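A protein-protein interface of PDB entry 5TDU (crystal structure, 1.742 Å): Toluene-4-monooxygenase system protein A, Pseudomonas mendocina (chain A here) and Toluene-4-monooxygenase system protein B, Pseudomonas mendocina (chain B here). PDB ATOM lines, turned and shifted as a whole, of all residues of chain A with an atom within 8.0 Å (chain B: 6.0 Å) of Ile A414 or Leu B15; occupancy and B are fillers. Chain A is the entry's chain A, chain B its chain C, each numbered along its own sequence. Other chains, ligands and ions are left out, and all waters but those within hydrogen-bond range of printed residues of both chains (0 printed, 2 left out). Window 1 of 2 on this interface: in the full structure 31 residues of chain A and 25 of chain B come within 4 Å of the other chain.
OG of Ser A330 is in hydrogen-bond range of O of Gly A406 (2.7 Å). The indole nitrogen (NE1) of Trp A338 lies within hydrogen-bond range of the backbone carbonyl oxygen (O) of Thr A392. N of Leu A404 is in hydrogen-bond range of O of Ser A395. The guanidinium group (NE) of Arg B42 is in salt-bridge range of the side-chain carboxylate (OD1) of Asp B13 (2.8 Å). The side-chain amide nitrogen of Gln B17 sits close to the guanidinium group of Arg B42 (3.3 Å). The backbone NH (N) of Arg B56 is in hydrogen-bond range of the side-chain carboxylate (OD2) of Asp B79.
Hydrophobic or aromatic side chains of chain A that line the printed part of chain B: Met A333, Tyr A337, Trp A338, Pro A394, Val A405, Pro A408, Trp A412, Ile A414 and Val A416. Among the printed residues, 32 pairs touch across the chains. Among the printed residues, Asp or Glu carboxylates within 4 Å of a Lys or Arg side-chain nitrogen of the other chain: Glu A415 with Arg B56 (3.8 Å).
The side-chain sulfur (SG) of Cys A372 lies close to the backbone carbonyl oxygen (O) of Arg B42, 3.5 Å away. N of Ser A395 is in hydrogen-bond range of O of Val B16 (2.9 Å). The backbone carbonyl oxygen (O) of Gln B17 sits close to the side-chain hydroxyl (OG) of Ser A395 (3.4 Å). The backbone carbonyl oxygen of Leu A404 is in hydrogen-bond range of the backbone NH of Val B16, at 2.9 Å. N of Gly A406 lies within hydrogen-bond range of O of Phe B14, at 2.9 Å. NE1 of Trp A412 lies within hydrogen-bond range of O of Phe B10 (3.4 Å). The indole nitrogen (NE1) of Trp A412 lies close to the backbone carbonyl oxygen (O) of Asp B13 (3.2 Å). The side-chain amide oxygen (OD1) of Asn A413 sits at hydrogen-bond distance from the guanidinium group (NH2) of Arg B56, 2.6 Å away. The backbone carbonyl oxygen (O) of Ile A414 sits at hydrogen-bond distance from the guanidinium group (NE) of Arg B56 (3.3 Å). NH1 of Arg B56 lies within salt-bridge range of OE1 of Glu A415, at 3.8 Å. A ring nitrogen (NE2) of His B55 lies within hydrogen-bond range of the backbone NH (N) of Val A416 (2.8 Å).
Among the printed residues, merely in contact across the chains: Ser A330 with Phe B14 (3.1 Å), Met A333 with Phe B14 (3.5 Å), Gly A334 with Phe B14 (3.5 Å), Tyr A337 with Arg B42 (3.3 Å), Trp A338 with Leu B15 (3.6 Å), Trp A338 with Gln B17 (3.2 Å), Thr A392 with Gln B17 (3.7 Å), Leu A393 with Gln B17 (3.8 Å), Pro A394 with Leu B15 (3.8 Å), Pro A394 with Val B16 (3.8 Å), Leu A404 with Leu B15 (3.3 Å), Val A405 with Phe B14 (3.2 Å), Pro A408 with Asp B13 (3.4 Å), Pro A408 with Phe B14 (3.8 Å), Ile A414 with Ala B9 (3.9 Å), Ile A414 with Phe B14 (3.96 Å), Ile A414 with Leu B15 (3.5 Å), Ile A414 with Val B16 (3.5 Å), Ile A414 with His B55 (3.3 Å), Glu A415 with His B55 (3.5 Å) and Val A416 with Val B16 (3.7 Å).
Ile A414 touches six residues of chain B. Of chain A, only Trp A338, Pro A394, Leu A404 and Ile A414 come within 4 Å of Leu B15. Printed residues of chain B within 4 Å of Ser A395: Val B16 (2.9 Å) and Gln B17 (3.1 Å). Of the printed residues of chain B, Pro A394 touches Leu B15 and Val B16. Pro A403 touches none of the printed residues of chain B. The nearest printed residue of chain B that does not touch Trp A338 is Arg B42 (4.2 Å).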
ATOM      1  N   SER A 330      -7.102  20.780   4.547  1.00  0.00           N
ATOM      2  CA  SER A 330      -8.235  20.933   5.452  1.00  0.00           C
ATOM      3  C   SER A 330      -9.559  20.544   4.802  1.00  0.00           C
ATOM      4  O   SER A 330     -10.422  19.958   5.454  1.00  0.00           O
ATOM      5  CB  SER A 330      -8.306  22.369   5.976  1.00  0.00           C
ATOM      6  OG  SER A 330      -7.414  22.537   7.064  1.00  0.00           O
ATOM      7  N   MET A 333      -9.705  16.845   5.000  1.00  0.00           N
ATOM      8  CA  MET A 333     -10.040  16.407   6.347  1.00  0.00           C
ATOM      9  C   MET A 333     -11.545  16.528   6.579  1.00  0.00           C
ATOM     10  O   MET A 333     -12.163  15.650   7.174  1.00  0.00           O
ATOM     11  CB  MET A 333      -9.266  17.222   7.380  1.00  0.00           C
ATOM     12  CG  MET A 333      -9.359  16.664   8.789  1.00  0.00           C
ATOM     13  SD  MET A 333      -8.251  17.531   9.907  1.00  0.00           S
ATOM     14  CE  MET A 333      -6.663  17.058   9.217  1.00  0.00           C
ATOM     15  N   GLY A 334     -12.133  17.613   6.084  1.00  0.00           N
ATOM     16  CA  GLY A 334     -13.559  17.839   6.244  1.00  0.00           C
ATOM     17  C   GLY A 334     -14.406  16.855   5.460  1.00  0.00           C
ATOM     18  O   GLY A 334     -15.403  16.334   5.959  1.00  0.00           O
ATOM     19  N   VAL A 335     -14.006  16.596   4.217  1.00  0.00           N
ATOM     20  CA  VAL A 335     -14.749  15.658   3.388  1.00  0.00           C
ATOM     21  C   VAL A 335     -14.671  14.267   4.001  1.00  0.00           C
ATOM     22  O   VAL A 335     -15.667  13.527   4.017  1.00  0.00           O
ATOM     23  CB  VAL A 335     -14.236  15.646   1.949  1.00  0.00           C
ATOM     24  CG1 VAL A 335     -14.824  14.451   1.191  1.00  0.00           C
ATOM     25  CG2 VAL A 335     -14.582  16.957   1.256  1.00  0.00           C
ATOM     26  N   TYR A 337     -13.988  13.414   7.306  1.00  0.00           N
ATOM     27  CA  TYR A 337     -14.657  13.272   8.602  1.00  0.00           C
ATOM     28  C   TYR A 337     -16.173  13.253   8.391  1.00  0.00           C
ATOM     29  O   TYR A 337     -16.882  12.502   9.052  1.00  0.00           O
ATOM     30  CB  TYR A 337     -14.256  14.381   9.577  1.00  0.00           C
ATOM     31  CG  TYR A 337     -14.527  14.001  11.023  1.00  0.00           C
ATOM     32  CD1 TYR A 337     -13.607  13.248  11.748  1.00  0.00           C
ATOM     33  CD2 TYR A 337     -15.712  14.370  11.646  1.00  0.00           C
ATOM     34  CE1 TYR A 337     -13.853  12.893  13.075  1.00  0.00           C
ATOM     35  CE2 TYR A 337     -15.968  14.009  12.973  1.00  0.00           C
ATOM     36  CZ  TYR A 337     -15.035  13.273  13.670  1.00  0.00           C
ATOM     37  OH  TYR A 337     -15.287  12.917  14.980  1.00  0.00           O
ATOM     38  N   TRP A 338     -16.659  14.051   7.440  1.00  0.00           N
ATOM     39  CA  TRP A 338     -18.086  14.068   7.111  1.00  0.00           C
ATOM     40  C   TRP A 338     -18.350  13.213   5.873  1.00  0.00           C
ATOM     41  O   TRP A 338     -19.271  13.487   5.099  1.00  0.00           O
ATOM     42  CB  TRP A 338     -18.595  15.509   6.901  1.00  0.00           C
ATOM     43  CG  TRP A 338     -18.975  16.199   8.199  1.00  0.00           C
ATOM     44  CD1 TRP A 338     -20.228  16.314   8.730  1.00  0.00           C
ATOM     45  CD2 TRP A 338     -18.090  16.855   9.110  1.00  0.00           C
ATOM     46  NE1 TRP A 338     -20.174  16.985   9.929  1.00  0.00           N
ATOM     47  CE2 TRP A 338     -18.874  17.333  10.183  1.00  0.00           C
ATOM     48  CE3 TRP A 338     -16.710  17.077   9.129  1.00  0.00           C
ATOM     49  CZ2 TRP A 338     -18.324  18.036  11.260  1.00  0.00           C
ATOM     50  CZ3 TRP A 338     -16.162  17.766  10.195  1.00  0.00           C
ATOM     51  CH2 TRP A 338     -16.971  18.230  11.258  1.00  0.00           C
ATOM     52  N   CYS A 372      -4.171  16.242  13.907  1.00  0.00           N
ATOM     53  CA  CYS A 372      -5.554  15.780  13.831  1.00  0.00           C
ATOM     54  C   CYS A 372      -5.633  14.307  13.435  1.00  0.00           C
ATOM     55  O   CYS A 372      -6.404  13.540  14.005  1.00  0.00           O
ATOM     56  CB  CYS A 372      -6.345  16.606  12.819  1.00  0.00           C
ATOM     57  SG  CYS A 372      -6.458  18.343  13.213  1.00  0.00           S
ATOM     58  N   THR A 392     -22.506  16.806  14.428  1.00  0.00           N
ATOM     59  CA  THR A 392     -23.025  18.126  14.102  1.00  0.00           C
ATOM     60  C   THR A 392     -22.639  18.476  12.669  1.00  0.00           C
ATOM     61  O   THR A 392     -22.014  17.666  11.979  1.00  0.00           O
ATOM     62  CB  THR A 392     -22.503  19.211  15.066  1.00  0.00           C
ATOM     63  OG1 THR A 392     -23.180  20.446  14.803  1.00  0.00           O
ATOM     64  CG2 THR A 392     -20.999  19.406  14.912  1.00  0.00           C
ATOM     65  N   LEU A 393     -23.026  19.670  12.227  1.00  0.00           N
ATOM     66  CA  LEU A 393     -22.684  20.143  10.884  1.00  0.00           C
ATOM     67  C   LEU A 393     -21.537  21.132  10.935  1.00  0.00           C
ATOM     68  O   LEU A 393     -21.414  21.905  11.888  1.00  0.00           O
ATOM     69  CB  LEU A 393     -23.886  20.803  10.206  1.00  0.00           C
ATOM     70  CG  LEU A 393     -25.060  19.928   9.779  1.00  0.00           C
ATOM     71  CD1 LEU A 393     -26.063  20.749   8.984  1.00  0.00           C
ATOM     72  CD2 LEU A 393     -24.565  18.741   8.974  1.00  0.00           C
ATOM     73  N   PRO A 394     -20.689  21.117   9.901  1.00  0.00           N
ATOM     74  CA  PRO A 394     -19.666  22.153   9.779  1.00  0.00           C
ATOM     75  C   PRO A 394     -20.314  23.491   9.432  1.00  0.00           C
ATOM     76  O   PRO A 394     -21.384  23.506   8.819  1.00  0.00           O
ATOM     77  CB  PRO A 394     -18.785  21.650   8.623  1.00  0.00           C
ATOM     78  CG  PRO A 394     -19.688  20.768   7.821  1.00  0.00           C
ATOM     79  CD  PRO A 394     -20.634  20.134   8.800  1.00  0.00           C
ATOM     80  N   SER A 395     -19.686  24.593   9.823  1.00  0.00           N
ATOM     81  CA  SER A 395     -20.130  25.910   9.379  1.00  0.00           C
ATOM     82  C   SER A 395     -19.699  26.067   7.929  1.00  0.00           C
ATOM     83  O   SER A 395     -18.634  25.593   7.563  1.00  0.00           O
ATOM     84  CB  SER A 395     -19.544  27.014  10.259  1.00  0.00           C
ATOM     85  OG  SER A 395     -19.836  26.762  11.634  1.00  0.00           O
ATOM     86  N   PRO A 403     -17.239  24.020   3.747  1.00  0.00           N
ATOM     87  CA  PRO A 403     -16.998  24.319   5.165  1.00  0.00           C
ATOM     88  C   PRO A 403     -15.865  25.320   5.427  1.00  0.00           C
ATOM     89  O   PRO A 403     -14.892  25.404   4.673  1.00  0.00           O
ATOM     90  CB  PRO A 403     -16.657  22.944   5.752  1.00  0.00           C
ATOM     91  CG  PRO A 403     -17.449  21.994   4.924  1.00  0.00           C
ATOM     92  CD  PRO A 403     -17.446  22.580   3.513  1.00  0.00           C
ATOM     93  N   LEU A 404     -16.008  26.071   6.517  1.00  0.00           N
ATOM     94  CA  LEU A 404     -15.033  27.076   6.939  1.00  0.00           C
ATOM     95  C   LEU A 404     -13.875  26.427   7.696  1.00  0.00           C
ATOM     96  O   LEU A 404     -14.076  25.838   8.760  1.00  0.00           O
ATOM     97  CB  LEU A 404     -15.720  28.131   7.821  1.00  0.00           C
ATOM     98  CG  LEU A 404     -16.930  28.872   7.228  1.00  0.00           C
ATOM     99  CD1 LEU A 404     -17.677  29.674   8.290  1.00  0.00           C
ATOM    100  CD2 LEU A 404     -16.485  29.798   6.090  1.00  0.00           C
ATOM    101  N   VAL A 405     -12.663  26.552   7.167  1.00  0.00           N
ATOM    102  CA  VAL A 405     -11.518  25.819   7.703  1.00  0.00           C
ATOM    103  C   VAL A 405     -10.327  26.736   7.975  1.00  0.00           C
ATOM    104  O   VAL A 405     -10.358  27.931   7.658  1.00  0.00           O
ATOM    105  CB  VAL A 405     -11.105  24.683   6.742  1.00  0.00           C
ATOM    106  CG1 VAL A 405     -12.256  23.711   6.546  1.00  0.00           C
ATOM    107  CG2 VAL A 405     -10.637  25.248   5.393  1.00  0.00           C
ATOM    108  N   GLY A 406      -9.277  26.156   8.550  1.00  0.00           N
ATOM    109  CA  GLY A 406      -8.028  26.852   8.798  1.00  0.00           C
ATOM    110  C   GLY A 406      -6.884  25.869   8.990  1.00  0.00           C
ATOM    111  O   GLY A 406      -6.985  24.714   8.594  1.00  0.00           O
ATOM    112  N   VAL A 407      -5.790  26.323   9.589  1.00  0.00           N
ATOM    113  CA  VAL A 407      -4.646  25.452   9.816  1.00  0.00           C
ATOM    114  C   VAL A 407      -4.731  24.901  11.231  1.00  0.00           C
ATOM    115  O   VAL A 407      -4.806  25.666  12.182  1.00  0.00           O
ATOM    116  CB  VAL A 407      -3.315  26.196   9.580  1.00  0.00           C
ATOM    117  CG1 VAL A 407      -2.121  25.307   9.958  1.00  0.00           C
ATOM    118  CG2 VAL A 407      -3.211  26.669   8.117  1.00  0.00           C
ATOM    119  N   PRO A 408      -4.744  23.566  11.375  1.00  0.00           N
ATOM    120  CA  PRO A 408      -4.848  22.955  12.706  1.00  0.00           C
ATOM    121  C   PRO A 408      -3.486  22.739  13.347  1.00  0.00           C
ATOM    122  O   PRO A 408      -2.463  23.062  12.748  1.00  0.00           O
ATOM    123  CB  PRO A 408      -5.516  21.613  12.408  1.00  0.00           C
ATOM    124  CG  PRO A 408      -4.964  21.245  11.050  1.00  0.00           C
ATOM    125  CD  PRO A 408      -4.756  22.549  10.302  1.00  0.00           C
ATOM    126  N   ASP A 411       0.629  25.392  15.109  1.00  0.00           N
ATOM    127  CA  ASP A 411       0.474  26.838  14.940  1.00  0.00           C
ATOM    128  C   ASP A 411      -0.915  27.166  14.398  1.00  0.00           C
ATOM    129  O   ASP A 411      -1.067  27.857  13.385  1.00  0.00           O
ATOM    130  CB  ASP A 411       1.577  27.412  14.048  1.00  0.00           C
ATOM    131  CG  ASP A 411       1.475  26.954  12.614  1.00  0.00           C
ATOM    132  OD1 ASP A 411       1.148  25.771  12.382  1.00  0.00           O
ATOM    133  OD2 ASP A 411       1.727  27.788  11.718  1.00  0.00           O
ATOM    134  N   TRP A 412      -1.918  26.655  15.109  1.00  0.00           N
ATOM    135  CA  TRP A 412      -3.332  26.887  14.834  1.00  0.00           C
ATOM    136  C   TRP A 412      -3.655  28.304  14.385  1.00  0.00           C
ATOM    137  O   TRP A 412      -3.257  29.275  15.023  1.00  0.00           O
ATOM    138  CB  TRP A 412      -4.149  26.564  16.091  1.00  0.00           C
ATOM    139  CG  TRP A 412      -5.645  26.718  15.953  1.00  0.00           C
ATOM    140  CD1 TRP A 412      -6.466  26.038  15.100  1.00  0.00           C
ATOM    141  CD2 TRP A 412      -6.500  27.573  16.732  1.00  0.00           C
ATOM    142  NE1 TRP A 412      -7.773  26.426  15.287  1.00  0.00           N
ATOM    143  CE2 TRP A 412      -7.819  27.369  16.280  1.00  0.00           C
ATOM    144  CE3 TRP A 412      -6.273  28.500  17.759  1.00  0.00           C
ATOM    145  CZ2 TRP A 412      -8.908  28.051  16.820  1.00  0.00           C
ATOM    146  CZ3 TRP A 412      -7.358  29.180  18.293  1.00  0.00           C
ATOM    147  CH2 TRP A 412      -8.657  28.954  17.821  1.00  0.00           C
ATOM    148  N   ASN A 413      -4.387  28.404  13.279  1.00  0.00           N
ATOM    149  CA  ASN A 413      -4.894  29.684  12.800  1.00  0.00           C
ATOM    150  C   ASN A 413      -6.107  29.465  11.911  1.00  0.00           C
ATOM    151  O   ASN A 413      -6.038  28.745  10.912  1.00  0.00           O
ATOM    152  CB  ASN A 413      -3.817  30.460  12.038  1.00  0.00           C
ATOM    153  CG  ASN A 413      -4.234  31.888  11.736  1.00  0.00           C
ATOM    154  OD1 ASN A 413      -4.178  32.753  12.603  1.00  0.00           O
ATOM    155  ND2 ASN A 413      -4.661  32.140  10.504  1.00  0.00           N
ATOM    156  N   ILE A 414      -7.223  30.079  12.280  1.00  0.00           N
ATOM    157  CA  ILE A 414      -8.430  29.976  11.480  1.00  0.00           C
ATOM    158  C   ILE A 414      -9.152  31.314  11.495  1.00  0.00           C
ATOM    159  O   ILE A 414      -9.305  31.938  12.545  1.00  0.00           O
ATOM    160  CB  ILE A 414      -9.328  28.827  11.980  1.00  0.00           C
ATOM    161  CG1 ILE A 414     -10.551  28.668  11.064  1.00  0.00           C
ATOM    162  CG2 ILE A 414      -9.716  29.036  13.451  1.00  0.00           C
ATOM    163  CD1 ILE A 414     -11.284  27.334  11.235  1.00  0.00           C
ATOM    164  N   GLU A 415      -9.563  31.780  10.319  1.00  0.00           N
ATOM    165  CA  GLU A 415     -10.279  33.041  10.242  1.00  0.00           C
ATOM    166  C   GLU A 415     -11.538  32.944   9.398  1.00  0.00           C
ATOM    167  O   GLU A 415     -11.529  32.393   8.294  1.00  0.00           O
ATOM    168  CB  GLU A 415      -9.385  34.150   9.691  1.00  0.00           C
ATOM    169  CG  GLU A 415     -10.069  35.522   9.739  1.00  0.00           C
ATOM    170  CD  GLU A 415      -9.098  36.688   9.639  1.00  0.00           C
ATOM    171  OE1 GLU A 415      -7.887  36.452   9.427  1.00  0.00           O
ATOM    172  OE2 GLU A 415      -9.553  37.847   9.784  1.00  0.00           O
ATOM    173  N   VAL A 416     -12.617  33.482   9.948  1.00  0.00           N
ATOM    174  CA  VAL A 416     -13.872  33.654   9.246  1.00  0.00           C
ATOM    175  C   VAL A 416     -14.004  35.135   8.895  1.00  0.00           C
ATOM    176  O   VAL A 416     -13.721  35.998   9.724  1.00  0.00           O
ATOM    177  CB  VAL A 416     -15.066  33.181  10.095  1.00  0.00           C
ATOM    178  CG1 VAL A 416     -16.384  33.420   9.353  1.00  0.00           C
ATOM    179  CG2 VAL A 416     -14.906  31.702  10.487  1.00  0.00           C
ATOM    180  N   PHE A 417     -14.429  35.428   7.671  1.00  0.00           N
ATOM    181  CA  PHE A 417     -14.608  36.811   7.235  1.00  0.00           C
ATOM    182  C   PHE A 417     -16.092  37.130   7.096  1.00  0.00           C
ATOM    183  O   PHE A 417     -16.744  36.705   6.151  1.00  0.00           O
ATOM    184  CB  PHE A 417     -13.846  37.045   5.926  1.00  0.00           C
ATOM    185  CG  PHE A 417     -12.374  36.791   6.061  1.00  0.00           C
ATOM    186  CD1 PHE A 417     -11.501  37.831   6.335  1.00  0.00           C
ATOM    187  CD2 PHE A 417     -11.871  35.500   5.981  1.00  0.00           C
ATOM    188  CE1 PHE A 417     -10.145  37.597   6.490  1.00  0.00           C
ATOM    189  CE2 PHE A 417     -10.514  35.260   6.129  1.00  0.00           C
ATOM    190  CZ  PHE A 417      -9.650  36.313   6.385  1.00  0.00           C
ATOM    191  N   GLY A 429     -15.297  32.165   3.900  1.00  0.00           N
ATOM    192  CA  GLY A 429     -14.078  31.449   4.222  1.00  0.00           C
ATOM    193  C   GLY A 429     -12.780  32.153   3.877  1.00  0.00           C
ATOM    194  O   GLY A 429     -11.700  31.619   4.120  1.00  0.00           O
ATOM    195  N   ALA B   8     -18.558  27.775  16.095  1.00  0.00           N
ATOM    196  CA  ALA B   8     -17.435  27.748  17.017  1.00  0.00           C
ATOM    197  C   ALA B   8     -16.174  27.144  16.433  1.00  0.00           C
ATOM    198  O   ALA B   8     -16.206  26.098  15.774  1.00  0.00           O
ATOM    199  CB  ALA B   8     -17.829  26.980  18.303  1.00  0.00           C
ATOM    200  N   ALA B   9     -15.053  27.793  16.721  1.00  0.00           N
ATOM    201  CA  ALA B   9     -13.739  27.292  16.328  1.00  0.00           C
ATOM    202  C   ALA B   9     -12.936  26.879  17.561  1.00  0.00           C
ATOM    203  O   ALA B   9     -12.647  27.717  18.418  1.00  0.00           O
ATOM    204  CB  ALA B   9     -12.989  28.349  15.529  1.00  0.00           C
ATOM    205  N   PHE B  10     -12.590  25.594  17.658  1.00  0.00           N
ATOM    206  CA  PHE B  10     -11.845  25.102  18.810  1.00  0.00           C
ATOM    207  C   PHE B  10     -10.339  25.126  18.556  1.00  0.00           C
ATOM    208  O   PHE B  10      -9.878  24.784  17.463  1.00  0.00           O
ATOM    209  CB  PHE B  10     -12.288  23.683  19.169  1.00  0.00           C
ATOM    210  CG  PHE B  10     -11.881  23.258  20.549  1.00  0.00           C
ATOM    211  CD1 PHE B  10     -10.586  22.823  20.805  1.00  0.00           C
ATOM    212  CD2 PHE B  10     -12.790  23.298  21.588  1.00  0.00           C
ATOM    213  CE1 PHE B  10     -10.208  22.428  22.082  1.00  0.00           C
ATOM    214  CE2 PHE B  10     -12.423  22.913  22.864  1.00  0.00           C
ATOM    215  CZ  PHE B  10     -11.129  22.479  23.111  1.00  0.00           C
ATOM    216  N   ASP B  13      -8.100  22.736  16.279  1.00  0.00           N
ATOM    217  CA  ASP B  13      -8.953  22.037  15.325  1.00  0.00           C
ATOM    218  C   ASP B  13      -8.734  22.648  13.938  1.00  0.00           C
ATOM    219  O   ASP B  13      -8.012  23.638  13.799  1.00  0.00           O
ATOM    220  CB  ASP B  13     -10.426  22.123  15.731  1.00  0.00           C
ATOM    221  CG  ASP B  13     -11.257  20.975  15.178  1.00  0.00           C
ATOM    222  OD1 ASP B  13     -10.704  20.132  14.428  1.00  0.00           O
ATOM    223  OD2 ASP B  13     -12.470  20.922  15.491  1.00  0.00           O
ATOM    224  N   PHE B  14      -9.349  22.056  12.915  1.00  0.00           N
ATOM    225  CA  PHE B  14      -9.151  22.516  11.540  1.00  0.00           C
ATOM    226  C   PHE B  14     -10.343  23.273  10.958  1.00  0.00           C
ATOM    227  O   PHE B  14     -10.261  23.774   9.829  1.00  0.00           O
ATOM    228  CB  PHE B  14      -8.831  21.326  10.633  1.00  0.00           C
ATOM    229  CG  PHE B  14     -10.049  20.608  10.125  1.00  0.00           C
ATOM    230  CD1 PHE B  14     -10.500  20.823   8.829  1.00  0.00           C
ATOM    231  CD2 PHE B  14     -10.742  19.718  10.937  1.00  0.00           C
ATOM    232  CE1 PHE B  14     -11.623  20.172   8.347  1.00  0.00           C
ATOM    233  CE2 PHE B  14     -11.867  19.056  10.461  1.00  0.00           C
ATOM    234  CZ  PHE B  14     -12.306  19.286   9.155  1.00  0.00           C
ATOM    235  N   LEU B  15     -11.444  23.369  11.701  1.00  0.00           N
ATOM    236  CA  LEU B  15     -12.626  24.008  11.134  1.00  0.00           C
ATOM    237  C   LEU B  15     -13.503  24.730  12.152  1.00  0.00           C
ATOM    238  O   LEU B  15     -13.237  24.729  13.370  1.00  0.00           O
ATOM    239  CB  LEU B  15     -13.481  22.978  10.378  1.00  0.00           C
ATOM    240  CG  LEU B  15     -14.508  22.190  11.201  1.00  0.00           C
ATOM    241  CD1 LEU B  15     -15.351  21.290  10.304  1.00  0.00           C
ATOM    242  CD2 LEU B  15     -13.819  21.377  12.287  1.00  0.00           C
ATOM    243  N   VAL B  16     -14.545  25.362  11.617  1.00  0.00           N
ATOM    244  CA  VAL B  16     -15.589  26.007  12.400  1.00  0.00           C
ATOM    245  C   VAL B  16     -16.830  25.137  12.303  1.00  0.00           C
ATOM    246  O   VAL B  16     -17.191  24.679  11.218  1.00  0.00           O
ATOM    247  CB  VAL B  16     -15.862  27.458  11.906  1.00  0.00           C
ATOM    248  CG1 VAL B  16     -16.864  28.163  12.799  1.00  0.00           C
ATOM    249  CG2 VAL B  16     -14.568  28.249  11.827  1.00  0.00           C
ATOM    250  N   GLN B  17     -17.469  24.869  13.445  1.00  0.00           N
ATOM    251  CA  GLN B  17     -18.640  24.003  13.444  1.00  0.00           C
ATOM    252  C   GLN B  17     -19.861  24.696  14.001  1.00  0.00           C
ATOM    253  O   GLN B  17     -19.756  25.588  14.848  1.00  0.00           O
ATOM    254  CB  GLN B  17     -18.390  22.732  14.268  1.00  0.00           C
ATOM    255  CG  GLN B  17     -17.407  21.750  13.676  1.00  0.00           C
ATOM    256  CD  GLN B  17     -17.102  20.613  14.635  1.00  0.00           C
ATOM    257  OE1 GLN B  17     -16.685  20.845  15.776  1.00  0.00           O
ATOM    258  NE2 GLN B  17     -17.321  19.385  14.188  1.00  0.00           N
ATOM    259  N   ARG B  42     -10.433  15.332  16.849  1.00  0.00           N
ATOM    260  CA  ARG B  42      -9.365  15.873  16.025  1.00  0.00           C
ATOM    261  C   ARG B  42      -8.375  16.663  16.871  1.00  0.00           C
ATOM    262  O   ARG B  42      -7.336  17.096  16.380  1.00  0.00           O
ATOM    263  CB  ARG B  42      -9.947  16.749  14.911  1.00  0.00           C
ATOM    264  CG  ARG B  42     -10.820  15.988  13.918  1.00  0.00           C
ATOM    265  CD  ARG B  42     -11.554  16.942  12.982  1.00  0.00           C
ATOM    266  NE  ARG B  42     -12.309  17.938  13.736  1.00  0.00           N
ATOM    267  CZ  ARG B  42     -13.546  17.764  14.194  1.00  0.00           C
ATOM    268  NH1 ARG B  42     -14.142  18.732  14.877  1.00  0.00           N
ATOM    269  NH2 ARG B  42     -14.188  16.628  13.973  1.00  0.00           N
ATOM    270  N   HIS B  55     -14.867  35.592  17.956  1.00  0.00           N
ATOM    271  CA  HIS B  55     -13.871  35.178  16.970  1.00  0.00           C
ATOM    272  C   HIS B  55     -12.736  36.189  16.826  1.00  0.00           C
ATOM    273  O   HIS B  55     -12.961  37.345  16.474  1.00  0.00           O
ATOM    274  CB  HIS B  55     -14.550  34.946  15.610  1.00  0.00           C
ATOM    275  CG  HIS B  55     -13.645  34.375  14.558  1.00  0.00           C
ATOM    276  ND1 HIS B  55     -12.828  33.287  14.780  1.00  0.00           N
ATOM    277  CD2 HIS B  55     -13.453  34.731  13.264  1.00  0.00           C
ATOM    278  CE1 HIS B  55     -12.161  33.005  13.674  1.00  0.00           C
ATOM    279  NE2 HIS B  55     -12.518  33.869  12.740  1.00  0.00           N
ATOM    280  N   ARG B  56     -11.515  35.739  17.106  1.00  0.00           N
ATOM    281  CA  ARG B  56     -10.314  36.543  16.881  1.00  0.00           C
ATOM    282  C   ARG B  56     -10.195  37.744  17.814  1.00  0.00           C
ATOM    283  O   ARG B  56      -9.355  38.619  17.591  1.00  0.00           O
ATOM    284  CB  ARG B  56     -10.267  37.038  15.432  1.00  0.00           C
ATOM    285  CG  ARG B  56     -10.289  35.941  14.392  1.00  0.00           C
ATOM    286  CD  ARG B  56      -9.277  36.213  13.292  1.00  0.00           C
ATOM    287  NE  ARG B  56      -8.405  35.062  13.115  1.00  0.00           N
ATOM    288  CZ  ARG B  56      -7.089  35.128  12.957  1.00  0.00           C
ATOM    289  NH1 ARG B  56      -6.478  36.302  12.941  1.00  0.00           N
ATOM    290  NH2 ARG B  56      -6.386  34.013  12.805  1.00  0.00           N
ATOM    291  N   ASP B  79     -14.590  31.607  19.414  1.00  0.00           N
ATOM    292  CA  ASP B  79     -13.469  30.688  19.568  1.00  0.00           C
ATOM    293  C   ASP B  79     -13.538  30.057  20.949  1.00  0.00           C
ATOM    294  O   ASP B  79     -14.053  30.674  21.878  1.00  0.00           O
ATOM    295  CB  ASP B  79     -12.122  31.397  19.420  1.00  0.00           C
ATOM    296  CG  ASP B  79     -11.960  32.094  18.083  1.00  0.00           C
ATOM    297  OD1 ASP B  79     -12.586  31.663  17.091  1.00  0.00           O
ATOM    298  OD2 ASP B  79     -11.186  33.070  18.031  1.00  0.00           O
